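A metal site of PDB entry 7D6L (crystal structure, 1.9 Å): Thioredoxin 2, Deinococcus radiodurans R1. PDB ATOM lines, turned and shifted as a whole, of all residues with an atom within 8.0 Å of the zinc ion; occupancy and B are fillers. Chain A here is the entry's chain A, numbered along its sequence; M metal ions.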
ATOM      1  N   THR A  12      -7.780 -27.357 -18.015  1.00  0.00           N
ATOM      2  CA  THR A  12      -8.967 -27.083 -17.206  1.00  0.00           C
ATOM      3  C   THR A  12      -8.628 -27.159 -15.725  1.00  0.00           C
ATOM      4  O   THR A  12      -8.034 -28.142 -15.256  1.00  0.00           O
ATOM      5  CB  THR A  12     -10.090 -28.051 -17.565  1.00  0.00           C
ATOM      6  OG1 THR A  12     -10.413 -27.861 -18.952  1.00  0.00           O
ATOM      7  CG2 THR A  12     -11.349 -27.768 -16.745  1.00  0.00           C
ATOM      8  N   CYS A  13      -8.987 -26.115 -14.992  1.00  0.00           N
ATOM      9  CA  CYS A  13      -8.643 -26.034 -13.582  1.00  0.00           C
ATOM     10  C   CYS A  13      -9.454 -27.078 -12.807  1.00  0.00           C
ATOM     11  O   CYS A  13     -10.678 -27.196 -12.984  1.00  0.00           O
ATOM     12  CB  CYS A  13      -8.919 -24.618 -13.060  1.00  0.00           C
ATOM     13  SG  CYS A  13      -8.684 -24.520 -11.287  1.00  0.00           S
ATOM     14  N   THR A  14      -8.783 -27.858 -11.968  1.00  0.00           N
ATOM     15  CA  THR A  14      -9.476 -28.905 -11.230  1.00  0.00           C
ATOM     16  C   THR A  14     -10.378 -28.304 -10.167  1.00  0.00           C
ATOM     17  O   THR A  14     -11.393 -28.918  -9.778  1.00  0.00           O
ATOM     18  CB  THR A  14      -8.456 -29.835 -10.582  1.00  0.00           C
ATOM     19  OG1 THR A  14      -7.641 -30.414 -11.608  1.00  0.00           O
ATOM     20  CG2 THR A  14      -9.132 -30.967  -9.822  1.00  0.00           C
ATOM     21  N   HIS A  15     -10.055 -27.087  -9.727  1.00  0.00           N
ATOM     22  CA  HIS A  15     -10.710 -26.527  -8.560  1.00  0.00           C
ATOM     23  C   HIS A  15     -11.912 -25.674  -8.945  1.00  0.00           C
ATOM     24  O   HIS A  15     -12.998 -25.864  -8.399  1.00  0.00           O
ATOM     25  CB  HIS A  15      -9.701 -25.738  -7.730  1.00  0.00           C
ATOM     26  CG  HIS A  15      -8.728 -26.608  -7.025  1.00  0.00           C
ATOM     27  ND1 HIS A  15      -7.512 -26.961  -7.570  1.00  0.00           N
ATOM     28  CD2 HIS A  15      -8.819 -27.277  -5.849  1.00  0.00           C
ATOM     29  CE1 HIS A  15      -6.883 -27.772  -6.739  1.00  0.00           C
ATOM     30  NE2 HIS A  15      -7.667 -27.987  -5.689  1.00  0.00           N
ATOM     31  N   CYS A  16     -11.786 -24.768  -9.904  1.00  0.00           N
ATOM     32  CA  CYS A  16     -12.896 -23.884 -10.230  1.00  0.00           C
ATOM     33  C   CYS A  16     -13.491 -24.112 -11.607  1.00  0.00           C
ATOM     34  O   CYS A  16     -14.427 -23.394 -11.966  1.00  0.00           O
ATOM     35  CB  CYS A  16     -12.453 -22.430 -10.107  1.00  0.00           C
ATOM     36  SG  CYS A  16     -11.431 -21.920 -11.539  1.00  0.00           S
ATOM     37  N   GLN A  17     -12.951 -25.065 -12.374  1.00  0.00           N
ATOM     38  CA  GLN A  17     -13.399 -25.457 -13.711  1.00  0.00           C
ATOM     39  C   GLN A  17     -12.999 -24.487 -14.806  1.00  0.00           C
ATOM     40  O   GLN A  17     -13.386 -24.706 -15.971  1.00  0.00           O
ATOM     41  CB  GLN A  17     -14.926 -25.624 -13.782  1.00  0.00           C
ATOM     42  CG  GLN A  17     -15.448 -26.686 -12.836  1.00  0.00           C
ATOM     43  CD  GLN A  17     -14.712 -27.976 -13.042  1.00  0.00           C
ATOM     44  OE1 GLN A  17     -14.087 -28.509 -12.143  1.00  0.00           O
ATOM     45  NE2 GLN A  17     -14.766 -28.474 -14.270  1.00  0.00           N
ATOM     46  N   ALA A  18     -12.270 -23.421 -14.496  1.00  0.00           N
ATOM     47  CA  ALA A  18     -11.924 -22.461 -15.530  1.00  0.00           C
ATOM     48  C   ALA A  18     -11.082 -23.136 -16.625  1.00  0.00           C
ATOM     49  O   ALA A  18     -10.120 -23.856 -16.340  1.00  0.00           O
ATOM     50  CB  ALA A  18     -11.148 -21.280 -14.919  1.00  0.00           C
ATOM     51  N   LYS A  19     -11.464 -22.877 -17.883  1.00  0.00           N
ATOM     52  CA  LYS A  19     -10.647 -23.204 -19.034  1.00  0.00           C
ATOM     53  C   LYS A  19      -9.538 -22.173 -19.181  1.00  0.00           C
ATOM     54  O   LYS A  19      -9.805 -20.973 -19.213  1.00  0.00           O
ATOM     55  CB  LYS A  19     -11.498 -23.244 -20.308  1.00  0.00           C
ATOM     56  CG  LYS A  19     -12.478 -24.411 -20.318  1.00  0.00           C
ATOM     57  CD  LYS A  19     -13.082 -24.652 -21.687  1.00  0.00           C
ATOM     58  CE  LYS A  19     -14.208 -25.673 -21.602  1.00  0.00           C
ATOM     59  NZ  LYS A  19     -15.448 -25.063 -21.020  1.00  0.00           N
ATOM     60  N   ASN A  20      -8.288 -22.652 -19.259  1.00  0.00           N
ATOM     61  CA  ASN A  20      -7.100 -21.813 -19.299  1.00  0.00           C
ATOM     62  C   ASN A  20      -6.329 -22.159 -20.565  1.00  0.00           C
ATOM     63  O   ASN A  20      -5.791 -23.266 -20.665  1.00  0.00           O
ATOM     64  CB  ASN A  20      -6.219 -22.053 -18.081  1.00  0.00           C
ATOM     65  CG  ASN A  20      -6.719 -21.299 -16.854  1.00  0.00           C
ATOM     66  OD1 ASN A  20      -6.275 -20.181 -16.572  1.00  0.00           O
ATOM     67  ND2 ASN A  20      -7.656 -21.904 -16.126  1.00  0.00           N
ATOM     68  N   SER A  32      -0.672 -21.891 -13.929  1.00  0.00           N
ATOM     69  CA  SER A  32      -1.663 -21.781 -12.870  1.00  0.00           C
ATOM     70  C   SER A  32      -2.960 -21.151 -13.393  1.00  0.00           C
ATOM     71  O   SER A  32      -2.952 -20.397 -14.369  1.00  0.00           O
ATOM     72  CB  SER A  32      -1.091 -20.982 -11.694  1.00  0.00           C
ATOM     73  OG  SER A  32      -0.758 -19.688 -12.129  1.00  0.00           O
ATOM     74  N   CYS A  33      -4.075 -21.478 -12.733  1.00  0.00           N
ATOM     75  CA  CYS A  33      -5.390 -20.970 -13.134  1.00  0.00           C
ATOM     76  C   CYS A  33      -5.451 -19.460 -12.946  1.00  0.00           C
ATOM     77  O   CYS A  33      -5.113 -18.966 -11.875  1.00  0.00           O
ATOM     78  CB  CYS A  33      -6.500 -21.622 -12.269  1.00  0.00           C
ATOM     79  SG  CYS A  33      -8.136 -21.052 -12.781  1.00  0.00           S
ATOM     80  N   ALA A  34      -5.883 -18.747 -13.989  1.00  0.00           N
ATOM     81  CA  ALA A  34      -5.940 -17.293 -13.945  1.00  0.00           C
ATOM     82  C   ALA A  34      -7.155 -16.796 -13.152  1.00  0.00           C
ATOM     83  O   ALA A  34      -7.226 -15.601 -12.823  1.00  0.00           O
ATOM     84  CB  ALA A  34      -6.007 -16.729 -15.364  1.00  0.00           C
ATOM     85  N   ARG A  35      -8.115 -17.653 -12.860  1.00  0.00           N
ATOM     86  CA  ARG A  35      -9.284 -17.243 -12.104  1.00  0.00           C
ATOM     87  C   ARG A  35      -9.066 -17.433 -10.607  1.00  0.00           C
ATOM     88  O   ARG A  35      -9.350 -16.534  -9.812  1.00  0.00           O
ATOM     89  CB  ARG A  35     -10.505 -18.032 -12.572  1.00  0.00           C
ATOM     90  CG  ARG A  35     -11.791 -17.792 -11.786  1.00  0.00           C
ATOM     91  CD  ARG A  35     -13.009 -18.035 -12.698  1.00  0.00           C
ATOM     92  NE  ARG A  35     -12.814 -17.389 -13.995  1.00  0.00           N
ATOM     93  CZ  ARG A  35     -13.538 -16.368 -14.446  1.00  0.00           C
ATOM     94  NH1 ARG A  35     -14.523 -15.866 -13.708  1.00  0.00           N
ATOM     95  NH2 ARG A  35     -13.279 -15.849 -15.650  1.00  0.00           N
ATOM     96  N   CYS A  36      -8.567 -18.599 -10.228  1.00  0.00           N
ATOM     97  CA  CYS A  36      -8.455 -18.940  -8.808  1.00  0.00           C
ATOM     98  C   CYS A  36      -7.023 -19.118  -8.328  1.00  0.00           C
ATOM     99  O   CYS A  36      -6.817 -19.225  -7.122  1.00  0.00           O
ATOM    100  CB  CYS A  36      -9.275 -20.212  -8.503  1.00  0.00           C
ATOM    101  SG  CYS A  36      -8.511 -21.823  -8.989  1.00  0.00           S
ATOM    102  N   GLY A  37      -6.028 -19.185  -9.233  1.00  0.00           N
ATOM    103  CA  GLY A  37      -4.641 -19.320  -8.806  1.00  0.00           C
ATOM    104  C   GLY A  37      -4.100 -20.740  -8.650  1.00  0.00           C
ATOM    105  O   GLY A  37      -2.883 -20.913  -8.463  1.00  0.00           O
ATOM    106  N   ALA A  38      -4.954 -21.765  -8.661  1.00  0.00           N
ATOM    107  CA  ALA A  38      -4.468 -23.119  -8.401  1.00  0.00           C
ATOM    108  C   ALA A  38      -3.550 -23.607  -9.545  1.00  0.00           C
ATOM    109  O   ALA A  38      -3.739 -23.248 -10.713  1.00  0.00           O
ATOM    110  CB  ALA A  38      -5.657 -24.078  -8.264  1.00  0.00           C
ATOM    111  N   ALA A  39      -2.560 -24.426  -9.210  1.00  0.00           N
ATOM    112  CA  ALA A  39      -1.755 -25.063 -10.249  1.00  0.00           C
ATOM    113  C   ALA A  39      -2.629 -25.923 -11.143  1.00  0.00           C
ATOM    114  O   ALA A  39      -3.533 -26.626 -10.666  1.00  0.00           O
ATOM    115  CB  ALA A  39      -0.642 -25.922  -9.650  1.00  0.00           C
ATOM    116  N   LEU A  40      -2.372 -25.863 -12.443  1.00  0.00           N
ATOM    117  CA  LEU A  40      -3.161 -26.611 -13.417  1.00  0.00           C
ATOM    118  C   LEU A  40      -2.559 -27.998 -13.683  1.00  0.00           C
ATOM    119  O   LEU A  40      -1.335 -28.173 -13.591  1.00  0.00           O
ATOM    120  CB  LEU A  40      -3.238 -25.851 -14.744  1.00  0.00           C
ATOM    121  CG  LEU A  40      -4.035 -24.513 -14.625  1.00  0.00           C
ATOM    122  CD1 LEU A  40      -3.673 -23.555 -15.743  1.00  0.00           C
ATOM    123  CD2 LEU A  40      -5.518 -24.790 -14.672  1.00  0.00           C
HETATM  124 ZN    ZN M   1      -9.257 -22.274 -11.041  1.00  0.00          ZN
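The zinc ion is bound by SG of Cys 36.
The zinc ion is bound by SG of Cys 16 (2.3 Å).
The side-chain sulfur (SG) of Cys 13 binds the zinc ion, at 2.3 Å.
The side-chain sulfur (SG) of Cys 33 binds the zinc ion (2.4 Å).
The nearest printed residue that does not touch the zinc ion is Ala 18 (4.4 Å).
The backbone NH of Ala 38 lies close to the side-chain sulfur of Cys 36.
The side-chain sulfur (SG) of Cys 16 sits close to the backbone NH (N) of Ala 18, at 3.4 Å.
The backbone carbonyl oxygen (O) of Ala 18 is in hydrogen-bond range of the backbone NH (N) of Cys 13, at 2.9 Å.
The backbone NH of His 15 lies close to the side-chain sulfur of Cys 13, at 3.3 Å.
The backbone NH (N) of Arg 35 lies close to the side-chain sulfur (SG) of Cys 33, 3.4 Å away.
The backbone NH of Cys 33 lies within hydrogen-bond range of the backbone carbonyl oxygen of Ala 38.
The side-chain sulfur (SG) of Cys 33 lies close to the side-chain amide nitrogen (ND2) of Asn 20 (3.5 Å).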
